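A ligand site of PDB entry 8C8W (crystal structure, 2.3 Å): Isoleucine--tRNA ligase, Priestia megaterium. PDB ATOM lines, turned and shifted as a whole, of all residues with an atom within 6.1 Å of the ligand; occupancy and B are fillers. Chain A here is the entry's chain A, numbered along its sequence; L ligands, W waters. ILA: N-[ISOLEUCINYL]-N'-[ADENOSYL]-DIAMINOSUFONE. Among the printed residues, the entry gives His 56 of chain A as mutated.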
ATOM      1  N   GLY A  45     -28.962  14.522 -11.930  1.00  0.00           N
ATOM      2  CA  GLY A  45     -29.974  15.546 -11.967  1.00  0.00           C
ATOM      3  C   GLY A  45     -29.583  16.638 -12.948  1.00  0.00           C
ATOM      4  O   GLY A  45     -28.490  17.215 -12.854  1.00  0.00           O
ATOM      5  N   PRO A  46     -30.457  16.954 -13.897  1.00  0.00           N
ATOM      6  CA  PRO A  46     -30.082  17.868 -14.983  1.00  0.00           C
ATOM      7  C   PRO A  46     -30.173  19.311 -14.549  1.00  0.00           C
ATOM      8  O   PRO A  46     -31.274  19.802 -14.219  1.00  0.00           O
ATOM      9  CB  PRO A  46     -31.111  17.540 -16.072  1.00  0.00           C
ATOM     10  CG  PRO A  46     -32.329  17.132 -15.306  1.00  0.00           C
ATOM     11  CD  PRO A  46     -31.821  16.417 -14.063  1.00  0.00           C
ATOM     12  N   PRO A  47     -29.055  20.040 -14.533  1.00  0.00           N
ATOM     13  CA  PRO A  47     -29.114  21.470 -14.226  1.00  0.00           C
ATOM     14  C   PRO A  47     -29.960  22.217 -15.249  1.00  0.00           C
ATOM     15  O   PRO A  47     -29.937  21.905 -16.442  1.00  0.00           O
ATOM     16  CB  PRO A  47     -27.641  21.911 -14.287  1.00  0.00           C
ATOM     17  CG  PRO A  47     -26.855  20.640 -14.161  1.00  0.00           C
ATOM     18  CD  PRO A  47     -27.687  19.574 -14.797  1.00  0.00           C
ATOM     19  N   THR A  48     -30.710  23.213 -14.768  1.00  0.00           N
ATOM     20  CA  THR A  48     -31.488  24.059 -15.659  1.00  0.00           C
ATOM     21  C   THR A  48     -30.557  24.945 -16.478  1.00  0.00           C
ATOM     22  O   THR A  48     -29.665  25.597 -15.935  1.00  0.00           O
ATOM     23  CB  THR A  48     -32.468  24.934 -14.874  1.00  0.00           C
ATOM     24  OG1 THR A  48     -33.309  24.104 -14.068  1.00  0.00           O
ATOM     25  CG2 THR A  48     -33.334  25.742 -15.824  1.00  0.00           C
ATOM     26  N   ALA A  49     -30.771  24.974 -17.792  1.00  0.00           N
ATOM     27  CA  ALA A  49     -29.904  25.762 -18.680  1.00  0.00           C
ATOM     28  C   ALA A  49     -30.469  27.174 -18.863  1.00  0.00           C
ATOM     29  O   ALA A  49     -30.806  27.613 -19.970  1.00  0.00           O
ATOM     30  CB  ALA A  49     -29.728  25.048 -20.017  1.00  0.00           C
ATOM     31  N   ASN A  50     -30.559  27.902 -17.748  1.00  0.00           N
ATOM     32  CA  ASN A  50     -31.138  29.242 -17.726  1.00  0.00           C
ATOM     33  C   ASN A  50     -30.238  30.259 -17.044  1.00  0.00           C
ATOM     34  O   ASN A  50     -30.700  31.378 -16.763  1.00  0.00           O
ATOM     35  CB  ASN A  50     -32.499  29.233 -17.030  1.00  0.00           C
ATOM     36  CG  ASN A  50     -32.388  28.970 -15.538  1.00  0.00           C
ATOM     37  OD1 ASN A  50     -31.395  28.425 -15.067  1.00  0.00           O
ATOM     38  ND2 ASN A  50     -33.409  29.376 -14.783  1.00  0.00           N
ATOM     39  N   HIS A  56     -21.872  27.617  -5.715  1.00  0.00           N
ATOM     40  CA  HIS A  56     -22.784  26.761  -4.963  1.00  0.00           C
ATOM     41  C   HIS A  56     -23.125  25.488  -5.727  1.00  0.00           C
ATOM     42  O   HIS A  56     -23.366  24.447  -5.107  1.00  0.00           O
ATOM     43  CB  HIS A  56     -24.050  27.527  -4.599  1.00  0.00           C
ATOM     44  CG  HIS A  56     -24.722  28.200  -5.752  1.00  0.00           C
ATOM     45  ND1 HIS A  56     -24.147  29.238  -6.453  1.00  0.00           N
ATOM     46  CD2 HIS A  56     -25.944  27.999  -6.304  1.00  0.00           C
ATOM     47  CE1 HIS A  56     -24.982  29.638  -7.403  1.00  0.00           C
ATOM     48  NE2 HIS A  56     -26.076  28.912  -7.327  1.00  0.00           N
ATOM     49  N   HIS A  57     -23.113  25.540  -7.066  1.00  0.00           N
ATOM     50  CA  HIS A  57     -23.364  24.344  -7.873  1.00  0.00           C
ATOM     51  C   HIS A  57     -22.193  23.371  -7.863  1.00  0.00           C
ATOM     52  O   HIS A  57     -22.364  22.226  -8.285  1.00  0.00           O
ATOM     53  CB  HIS A  57     -23.670  24.739  -9.325  1.00  0.00           C
ATOM     54  CG  HIS A  57     -24.881  25.615  -9.476  1.00  0.00           C
ATOM     55  ND1 HIS A  57     -24.851  26.833 -10.116  1.00  0.00           N
ATOM     56  CD2 HIS A  57     -26.159  25.437  -9.063  1.00  0.00           C
ATOM     57  CE1 HIS A  57     -26.061  27.367 -10.101  1.00  0.00           C
ATOM     58  NE2 HIS A  57     -26.868  26.545  -9.466  1.00  0.00           N
ATOM     59  N   LEU A  59     -20.743  22.150  -5.221  1.00  0.00           N
ATOM     60  CA  LEU A  59     -20.849  21.191  -4.120  1.00  0.00           C
ATOM     61  C   LEU A  59     -21.478  19.893  -4.581  1.00  0.00           C
ATOM     62  O   LEU A  59     -20.919  18.809  -4.363  1.00  0.00           O
ATOM     63  CB  LEU A  59     -21.655  21.798  -2.966  1.00  0.00           C
ATOM     64  CG  LEU A  59     -21.980  20.851  -1.800  1.00  0.00           C
ATOM     65  CD1 LEU A  59     -20.705  20.372  -1.117  1.00  0.00           C
ATOM     66  CD2 LEU A  59     -22.923  21.513  -0.798  1.00  0.00           C
ATOM     67  N   GLY A  60     -22.640  19.967  -5.229  1.00  0.00           N
ATOM     68  CA  GLY A  60     -23.311  18.767  -5.676  1.00  0.00           C
ATOM     69  C   GLY A  60     -22.518  18.002  -6.724  1.00  0.00           C
ATOM     70  O   GLY A  60     -22.412  16.776  -6.652  1.00  0.00           O
ATOM     71  N   LYS A  64     -21.183  14.179  -6.314  1.00  0.00           N
ATOM     72  CA  LYS A  64     -21.508  13.141  -7.284  1.00  0.00           C
ATOM     73  C   LYS A  64     -20.241  12.531  -7.882  1.00  0.00           C
ATOM     74  O   LYS A  64     -20.142  11.315  -8.030  1.00  0.00           O
ATOM     75  CB  LYS A  64     -22.404  13.716  -8.383  1.00  0.00           C
ATOM     76  CG  LYS A  64     -23.793  14.091  -7.905  1.00  0.00           C
ATOM     77  CD  LYS A  64     -24.694  14.578  -9.032  1.00  0.00           C
ATOM     78  CE  LYS A  64     -24.499  16.057  -9.314  1.00  0.00           C
ATOM     79  NZ  LYS A  64     -25.537  16.554 -10.263  1.00  0.00           N
ATOM     80  N   ASP A  85     -31.645  20.351 -18.310  1.00  0.00           N
ATOM     81  CA  ASP A  85     -33.056  20.684 -18.176  1.00  0.00           C
ATOM     82  C   ASP A  85     -33.313  21.973 -18.969  1.00  0.00           C
ATOM     83  O   ASP A  85     -32.715  23.012 -18.670  1.00  0.00           O
ATOM     84  CB  ASP A  85     -33.402  20.870 -16.706  1.00  0.00           C
ATOM     85  CG  ASP A  85     -34.810  20.417 -16.360  1.00  0.00           C
ATOM     86  OD1 ASP A  85     -35.584  20.095 -17.289  1.00  0.00           O
ATOM     87  OD2 ASP A  85     -35.135  20.381 -15.154  1.00  0.00           O
ATOM     88  N   TRP A 130     -22.112  25.528 -18.704  1.00  0.00           N
ATOM     89  CA  TRP A 130     -22.142  24.475 -17.694  1.00  0.00           C
ATOM     90  C   TRP A 130     -21.148  23.365 -18.025  1.00  0.00           C
ATOM     91  O   TRP A 130     -20.464  22.848 -17.128  1.00  0.00           O
ATOM     92  CB  TRP A 130     -23.551  23.913 -17.566  1.00  0.00           C
ATOM     93  CG  TRP A 130     -24.391  24.694 -16.597  1.00  0.00           C
ATOM     94  CD1 TRP A 130     -25.086  25.830 -16.861  1.00  0.00           C
ATOM     95  CD2 TRP A 130     -24.618  24.393 -15.220  1.00  0.00           C
ATOM     96  NE1 TRP A 130     -25.739  26.264 -15.722  1.00  0.00           N
ATOM     97  CE2 TRP A 130     -25.459  25.400 -14.704  1.00  0.00           C
ATOM     98  CE3 TRP A 130     -24.173  23.371 -14.367  1.00  0.00           C
ATOM     99  CZ2 TRP A 130     -25.880  25.400 -13.379  1.00  0.00           C
ATOM    100  CZ3 TRP A 130     -24.593  23.382 -13.050  1.00  0.00           C
ATOM    101  CH2 TRP A 130     -25.441  24.391 -12.570  1.00  0.00           C
ATOM    102  N   TRP A 517     -41.081  20.069 -14.050  1.00  0.00           N
ATOM    103  CA  TRP A 517     -40.632  19.024 -13.131  1.00  0.00           C
ATOM    104  C   TRP A 517     -40.977  17.637 -13.651  1.00  0.00           C
ATOM    105  O   TRP A 517     -40.279  16.671 -13.317  1.00  0.00           O
ATOM    106  CB  TRP A 517     -41.249  19.248 -11.746  1.00  0.00           C
ATOM    107  CG  TRP A 517     -40.659  20.410 -11.039  1.00  0.00           C
ATOM    108  CD1 TRP A 517     -41.286  21.585 -10.739  1.00  0.00           C
ATOM    109  CD2 TRP A 517     -39.315  20.534 -10.552  1.00  0.00           C
ATOM    110  NE1 TRP A 517     -40.418  22.432 -10.091  1.00  0.00           N
ATOM    111  CE2 TRP A 517     -39.206  21.808  -9.963  1.00  0.00           C
ATOM    112  CE3 TRP A 517     -38.207  19.686 -10.552  1.00  0.00           C
ATOM    113  CZ2 TRP A 517     -38.018  22.255  -9.383  1.00  0.00           C
ATOM    114  CZ3 TRP A 517     -37.025  20.137  -9.980  1.00  0.00           C
ATOM    115  CH2 TRP A 517     -36.945  21.408  -9.398  1.00  0.00           C
ATOM    116  N   SER A 520     -37.959  16.317 -15.893  1.00  0.00           N
ATOM    117  CA  SER A 520     -36.808  15.784 -15.184  1.00  0.00           C
ATOM    118  C   SER A 520     -37.161  14.545 -14.374  1.00  0.00           C
ATOM    119  O   SER A 520     -36.340  13.627 -14.259  1.00  0.00           O
ATOM    120  CB  SER A 520     -36.199  16.860 -14.277  1.00  0.00           C
ATOM    121  OG  SER A 520     -37.142  17.302 -13.306  1.00  0.00           O
ATOM    122  N   ALA A 548     -27.818  12.556  -5.754  1.00  0.00           N
ATOM    123  CA  ALA A 548     -27.270  13.566  -4.848  1.00  0.00           C
ATOM    124  C   ALA A 548     -27.551  14.944  -5.429  1.00  0.00           C
ATOM    125  O   ALA A 548     -26.942  15.324  -6.434  1.00  0.00           O
ATOM    126  CB  ALA A 548     -25.777  13.355  -4.618  1.00  0.00           C
ATOM    127  N   GLU A 549     -28.469  15.678  -4.803  1.00  0.00           N
ATOM    128  CA  GLU A 549     -28.837  17.024  -5.238  1.00  0.00           C
ATOM    129  C   GLU A 549     -29.187  17.842  -4.000  1.00  0.00           C
ATOM    130  O   GLU A 549     -29.224  17.328  -2.876  1.00  0.00           O
ATOM    131  CB  GLU A 549     -30.018  16.991  -6.238  1.00  0.00           C
ATOM    132  CG  GLU A 549     -29.809  16.119  -7.476  1.00  0.00           C
ATOM    133  CD  GLU A 549     -28.729  16.657  -8.422  1.00  0.00           C
ATOM    134  OE1 GLU A 549     -28.517  17.892  -8.449  1.00  0.00           O
ATOM    135  OE2 GLU A 549     -28.104  15.853  -9.131  1.00  0.00           O
ATOM    136  N   GLY A 550     -29.481  19.126  -4.211  1.00  0.00           N
ATOM    137  CA  GLY A 550     -29.754  20.011  -3.094  1.00  0.00           C
ATOM    138  C   GLY A 550     -31.110  19.750  -2.460  1.00  0.00           C
ATOM    139  O   GLY A 550     -32.031  19.217  -3.071  1.00  0.00           O
ATOM    140  N   ILE A 551     -31.231  20.196  -1.206  1.00  0.00           N
ATOM    141  CA  ILE A 551     -32.418  19.947  -0.384  1.00  0.00           C
ATOM    142  C   ILE A 551     -33.683  20.487  -1.029  1.00  0.00           C
ATOM    143  O   ILE A 551     -34.782  20.002  -0.734  1.00  0.00           O
ATOM    144  CB  ILE A 551     -32.217  20.552   1.030  1.00  0.00           C
ATOM    145  CG1 ILE A 551     -33.359  20.151   1.972  1.00  0.00           C
ATOM    146  CG2 ILE A 551     -32.106  22.066   0.951  1.00  0.00           C
ATOM    147  CD1 ILE A 551     -33.230  20.709   3.376  1.00  0.00           C
ATOM    148  N   ASP A 552     -33.563  21.482  -1.907  1.00  0.00           N
ATOM    149  CA  ASP A 552     -34.747  22.020  -2.574  1.00  0.00           C
ATOM    150  C   ASP A 552     -35.424  20.986  -3.462  1.00  0.00           C
ATOM    151  O   ASP A 552     -36.603  21.143  -3.798  1.00  0.00           O
ATOM    152  CB  ASP A 552     -34.365  23.262  -3.391  1.00  0.00           C
ATOM    153  CG  ASP A 552     -33.091  23.060  -4.195  1.00  0.00           C
ATOM    154  OD1 ASP A 552     -32.055  22.670  -3.611  1.00  0.00           O
ATOM    155  OD2 ASP A 552     -33.121  23.284  -5.429  1.00  0.00           O
ATOM    156  N   GLN A 553     -34.717  19.918  -3.851  1.00  0.00           N
ATOM    157  CA  GLN A 553     -35.340  18.900  -4.677  1.00  0.00           C
ATOM    158  C   GLN A 553     -36.356  18.051  -3.910  1.00  0.00           C
ATOM    159  O   GLN A 553     -37.136  17.339  -4.556  1.00  0.00           O
ATOM    160  CB  GLN A 553     -34.262  18.001  -5.304  1.00  0.00           C
ATOM    161  CG  GLN A 553     -33.176  18.759  -6.050  1.00  0.00           C
ATOM    162  CD  GLN A 553     -33.710  19.744  -7.083  1.00  0.00           C
ATOM    163  OE1 GLN A 553     -34.760  19.518  -7.684  1.00  0.00           O
ATOM    164  NE2 GLN A 553     -32.985  20.826  -7.292  1.00  0.00           N
ATOM    165  N   TRP A 557     -36.947  17.685  -7.889  1.00  0.00           N
ATOM    166  CA  TRP A 557     -36.596  16.470  -8.609  1.00  0.00           C
ATOM    167  C   TRP A 557     -36.817  15.219  -7.757  1.00  0.00           C
ATOM    168  O   TRP A 557     -37.265  14.195  -8.273  1.00  0.00           O
ATOM    169  CB  TRP A 557     -35.144  16.556  -9.079  1.00  0.00           C
ATOM    170  CG  TRP A 557     -34.745  15.531 -10.092  1.00  0.00           C
ATOM    171  CD1 TRP A 557     -35.379  15.252 -11.282  1.00  0.00           C
ATOM    172  CD2 TRP A 557     -33.609  14.666 -10.042  1.00  0.00           C
ATOM    173  NE1 TRP A 557     -34.710  14.263 -11.954  1.00  0.00           N
ATOM    174  CE2 TRP A 557     -33.610  13.887 -11.222  1.00  0.00           C
ATOM    175  CE3 TRP A 557     -32.585  14.472  -9.105  1.00  0.00           C
ATOM    176  CZ2 TRP A 557     -32.637  12.928 -11.488  1.00  0.00           C
ATOM    177  CZ3 TRP A 557     -31.606  13.521  -9.372  1.00  0.00           C
ATOM    178  CH2 TRP A 557     -31.645  12.761 -10.553  1.00  0.00           C
ATOM    179  N   LEU A 580     -28.476  17.630  -0.120  1.00  0.00           N
ATOM    180  CA  LEU A 580     -27.348  18.507   0.181  1.00  0.00           C
ATOM    181  C   LEU A 580     -27.831  19.877   0.633  1.00  0.00           C
ATOM    182  O   LEU A 580     -28.748  20.453   0.037  1.00  0.00           O
ATOM    183  CB  LEU A 580     -26.446  18.661  -1.041  1.00  0.00           C
ATOM    184  CG  LEU A 580     -26.020  17.322  -1.637  1.00  0.00           C
ATOM    185  CD1 LEU A 580     -25.179  17.522  -2.885  1.00  0.00           C
ATOM    186  CD2 LEU A 580     -25.282  16.495  -0.599  1.00  0.00           C
ATOM    187  N   GLY A 581     -27.203  20.391   1.688  1.00  0.00           N
ATOM    188  CA  GLY A 581     -27.491  21.733   2.126  1.00  0.00           C
ATOM    189  C   GLY A 581     -26.964  22.768   1.149  1.00  0.00           C
ATOM    190  O   GLY A 581     -26.099  22.491   0.319  1.00  0.00           O
ATOM    191  N   HIS A 582     -27.498  23.977   1.246  1.00  0.00           N
ATOM    192  CA  HIS A 582     -27.178  25.026   0.298  1.00  0.00           C
ATOM    193  C   HIS A 582     -25.956  25.815   0.726  1.00  0.00           C
ATOM    194  O   HIS A 582     -25.746  26.059   1.924  1.00  0.00           O
ATOM    195  CB  HIS A 582     -28.375  25.963   0.099  1.00  0.00           C
ATOM    196  CG  HIS A 582     -29.372  25.453  -0.889  1.00  0.00           C
ATOM    197  ND1 HIS A 582     -30.423  26.211  -1.357  1.00  0.00           N
ATOM    198  CD2 HIS A 582     -29.477  24.238  -1.504  1.00  0.00           C
ATOM    199  CE1 HIS A 582     -31.129  25.498  -2.209  1.00  0.00           C
ATOM    200  NE2 HIS A 582     -30.583  24.303  -2.322  1.00  0.00           N
ATOM    201  N   VAL A 583     -25.144  26.204  -0.253  1.00  0.00           N
ATOM    202  CA  VAL A 583     -23.973  27.039  -0.034  1.00  0.00           C
ATOM    203  C   VAL A 583     -24.413  28.487   0.126  1.00  0.00           C
ATOM    204  O   VAL A 583     -25.260  28.979  -0.633  1.00  0.00           O
ATOM    205  CB  VAL A 583     -22.976  26.880  -1.202  1.00  0.00           C
ATOM    206  CG1 VAL A 583     -21.806  27.825  -1.035  1.00  0.00           C
ATOM    207  CG2 VAL A 583     -22.501  25.437  -1.292  1.00  0.00           C
ATOM    208  N   LEU A 584     -23.847  29.171   1.124  1.00  0.00           N
ATOM    209  CA  LEU A 584     -24.179  30.551   1.453  1.00  0.00           C
ATOM    210  C   LEU A 584     -22.966  31.462   1.218  1.00  0.00           C
ATOM    211  O   LEU A 584     -21.829  30.992   1.141  1.00  0.00           O
ATOM    212  CB  LEU A 584     -24.639  30.671   2.909  1.00  0.00           C
ATOM    213  CG  LEU A 584     -25.610  29.592   3.377  1.00  0.00           C
ATOM    214  CD1 LEU A 584     -25.912  29.742   4.851  1.00  0.00           C
ATOM    215  CD2 LEU A 584     -26.890  29.641   2.562  1.00  0.00           C
ATOM    216  N   GLN A 589     -28.284  33.040   0.586  1.00  0.00           N
ATOM    217  CA  GLN A 589     -28.170  31.838  -0.217  1.00  0.00           C
ATOM    218  C   GLN A 589     -27.698  32.186  -1.623  1.00  0.00           C
ATOM    219  O   GLN A 589     -28.288  33.047  -2.283  1.00  0.00           O
ATOM    220  CB  GLN A 589     -29.498  31.092  -0.272  1.00  0.00           C
ATOM    221  CG  GLN A 589     -29.506  29.907  -1.232  1.00  0.00           C
ATOM    222  CD  GLN A 589     -30.885  29.282  -1.376  1.00  0.00           C
ATOM    223  OE1 GLN A 589     -31.386  29.110  -2.491  1.00  0.00           O
ATOM    224  NE2 GLN A 589     -31.498  28.930  -0.245  1.00  0.00           N
ATOM    225  N   LYS A 590     -26.642  31.513  -2.078  1.00  0.00           N
ATOM    226  CA  LYS A 590     -26.136  31.725  -3.430  1.00  0.00           C
ATOM    227  C   LYS A 590     -27.182  31.288  -4.452  1.00  0.00           C
ATOM    228  O   LYS A 590     -27.818  30.245  -4.318  1.00  0.00           O
ATOM    229  CB  LYS A 590     -24.835  30.959  -3.645  1.00  0.00           C
ATOM    230  CG  LYS A 590     -23.637  31.598  -2.976  1.00  0.00           C
ATOM    231  CD  LYS A 590     -22.363  30.885  -3.401  1.00  0.00           C
ATOM    232  CE  LYS A 590     -21.121  31.602  -2.889  1.00  0.00           C
ATOM    233  NZ  LYS A 590     -21.029  31.557  -1.409  1.00  0.00           N
ATOM    234  N   MET A 591     -27.326  32.105  -5.503  1.00  0.00           N
ATOM    235  CA  MET A 591     -28.419  31.979  -6.467  1.00  0.00           C
ATOM    236  C   MET A 591     -28.148  33.000  -7.569  1.00  0.00           C
ATOM    237  O   MET A 591     -27.183  33.765  -7.511  1.00  0.00           O
ATOM    238  CB  MET A 591     -29.761  32.223  -5.779  1.00  0.00           C
ATOM    239  CG  MET A 591     -30.998  31.748  -6.513  1.00  0.00           C
ATOM    240  SD  MET A 591     -32.492  32.519  -5.849  1.00  0.00           S
ATOM    241  CE  MET A 591     -33.746  31.482  -6.582  1.00  0.00           C
HETATM  242  N   ILA L   1     -33.043  21.379 -13.141  1.00  0.00           N
HETATM  243  CA  ILA L   1     -33.517  21.349 -11.763  1.00  0.00           C
HETATM  244  CB  ILA L   1     -33.474  19.947 -11.121  1.00  0.00           C
HETATM  245  CG2 ILA L   1     -34.230  18.939 -11.990  1.00  0.00           C
HETATM  246  CG1 ILA L   1     -32.032  19.521 -10.893  1.00  0.00           C
HETATM  247  CD  ILA L   1     -31.901  18.246 -10.064  1.00  0.00           C
HETATM  248  C   ILA L   1     -32.653  22.327 -10.978  1.00  0.00           C
HETATM  249  O   ILA L   1     -32.924  22.664  -9.841  1.00  0.00           O
HETATM  250  SA  ILA L   1     -30.440  23.901 -10.992  1.00  0.00           S
HETATM  251  O1A ILA L   1     -29.411  24.003 -11.984  1.00  0.00           O
HETATM  252  O2A ILA L   1     -31.164  25.064 -10.555  1.00  0.00           O
HETATM  253  N3A ILA L   1     -31.552  22.800 -11.635  1.00  0.00           N
HETATM  254  N5' ILA L   1     -29.768  23.215  -9.695  1.00  0.00           N
HETATM  255  C5' ILA L   1     -28.597  22.379  -9.860  1.00  0.00           C
HETATM  256  C4' ILA L   1     -28.242  21.702  -8.548  1.00  0.00           C
HETATM  257  O4' ILA L   1     -27.737  22.669  -7.630  1.00  0.00           O
HETATM  258  C1' ILA L   1     -28.471  22.649  -6.428  1.00  0.00           C
HETATM  259  N9  ILA L   1     -28.458  23.972  -5.850  1.00  0.00           N
HETATM  260  C4  ILA L   1     -27.679  24.391  -4.809  1.00  0.00           C
HETATM  261  N3  ILA L   1     -26.780  23.685  -4.117  1.00  0.00           N
HETATM  262  C2  ILA L   1     -26.206  24.409  -3.172  1.00  0.00           C
HETATM  263  N1  ILA L   1     -26.429  25.687  -2.871  1.00  0.00           N
HETATM  264  C6  ILA L   1     -27.328  26.380  -3.569  1.00  0.00           C
HETATM  265  N6  ILA L   1     -27.545  27.653  -3.261  1.00  0.00           N
HETATM  266  C5  ILA L   1     -28.009  25.719  -4.604  1.00  0.00           C
HETATM  267  N7  ILA L   1     -28.977  26.115  -5.495  1.00  0.00           N
HETATM  268  C8  ILA L   1     -29.214  25.057  -6.215  1.00  0.00           C
HETATM  269  C2' ILA L   1     -29.842  22.109  -6.821  1.00  0.00           C
HETATM  270  O2' ILA L   1     -30.503  21.601  -5.704  1.00  0.00           O
HETATM  271  C3' ILA L   1     -29.434  21.049  -7.846  1.00  0.00           C
HETATM  272  O3' ILA L   1     -28.979  19.913  -7.168  1.00  0.00           O
HETATM  273  O   HOH W   1     -24.892  20.837  -8.399  1.00  0.00           O
HETATM  274  O   HOH W   2     -28.226  19.102 -10.866  1.00  0.00           O
HETATM  275  O   HOH W   3     -29.809  27.443  -8.976  1.00  0.00           O
HETATM  276  O   HOH W   4     -29.230  26.552 -13.070  1.00  0.00           O
HETATM  277  O   HOH W   5     -24.628  22.058  -5.500  1.00  0.00           O
HETATM  278  O   HOH W   6     -32.149  24.600  -7.799  1.00  0.00           O
HETATM  279  O   HOH W   7     -36.752  22.380 -12.567  1.00  0.00           O
HETATM  280  O   HOH W   8     -33.284  27.427 -11.999  1.00  0.00           O
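An oxygen (O3') of the ligand lies within hydrogen-bond range of the side-chain carboxylate of Glu 549 (2.4 Å). The backbone carbonyl oxygen (O) of Pro 46 is in hydrogen-bond range of a nitrogen (N) of the ligand (2.6 Å). O of Lys 590 lies within hydrogen-bond range of N6 of the ligand (2.8 Å). An oxygen (O2') of the ligand lies within hydrogen-bond range of the side-chain carboxylate (OD1) of Asp 552 (2.8 Å). The backbone NH (N) of Thr 48 lies within hydrogen-bond range of an oxygen (O1A) of the ligand, 3.2 Å away. The side-chain hydroxyl (OG1) of Thr 48 is in hydrogen-bond range of a nitrogen (N) of the ligand. N1 of the ligand sits at hydrogen-bond distance from N of Val 583. NE2 of Gln 553 sits at hydrogen-bond distance from O2' of the ligand (3.0 Å). N of Gly 550 is in hydrogen-bond range of O2' of the ligand, 3.1 Å away. A nitrogen (N) of the ligand is in salt-bridge range of the side-chain carboxylate (OD2) of Asp 85, at 3.1 Å.
The backbone NH of Gly 45 is in hydrogen-bond range of the side-chain carboxylate of Glu 549, 3.2 Å away. The backbone NH of Leu 580 is in hydrogen-bond range of the backbone carbonyl oxygen of Glu 549 (2.9 Å). O of Leu 584 lies within hydrogen-bond range of NZ of Lys 590. The side-chain amide nitrogen of Gln 553 sits at hydrogen-bond distance from the side-chain carboxylate of Asp 552, 3.1 Å away. OE1 of Gln 553 is in hydrogen-bond range of N of Trp 557 (2.9 Å). A ring nitrogen (NE2) of His 57 lies close to a ring nitrogen (NE2) of His 56. The side-chain hydroxyl (OG) of Ser 520 is in hydrogen-bond range of the backbone carbonyl oxygen (O) of Trp 517. O of Ser 520 lies within hydrogen-bond range of NE1 of Trp 557 (2.9 Å).
Gly 45 touches the ligand. Pro 47 touches the ligand (CA to O1A, 3.4 Å). His 56 touches the ligand. His 57 touches the ligand (CD2 to O4', 3.5 Å). Trp 517 touches the ligand (CZ3 to CG2, 3.6 Å). Ser 520 touches the ligand. Trp 557 touches the ligand. Gly 581 touches the ligand. CA of His 582 touches N1 of the ligand (3.3 Å). Gln 589 touches the ligand. The nearest printed residue that does not touch the ligand is Trp 130 (4.03 Å).
Water W6 bridges the side-chain carboxylate (OD2) of Asp 552 and an oxygen (O) of the ligand. Water W5 lies within hydrogen-bond range of O of His 56 (2.7 Å), N of Gly 60 (2.9 Å) and N3 of the ligand (3.0 Å). Water W3 bridges NE2 of His 57 (3.1 Å) and O2A of the ligand (3.2 Å). Water W2 lies within hydrogen-bond range of OE1 of Glu 549 (2.7 Å) and O of Gly 45 (2.8 Å). Water W1 bridges the backbone carbonyl oxygen of His 57 (2.9 Å) and an oxygen (O4') of the ligand (3.5 Å). Water W8 bridges the side-chain amide nitrogen (ND2) of Asn 50 (3.4 Å) and an oxygen (O2A) of the ligand (3.5 Å).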
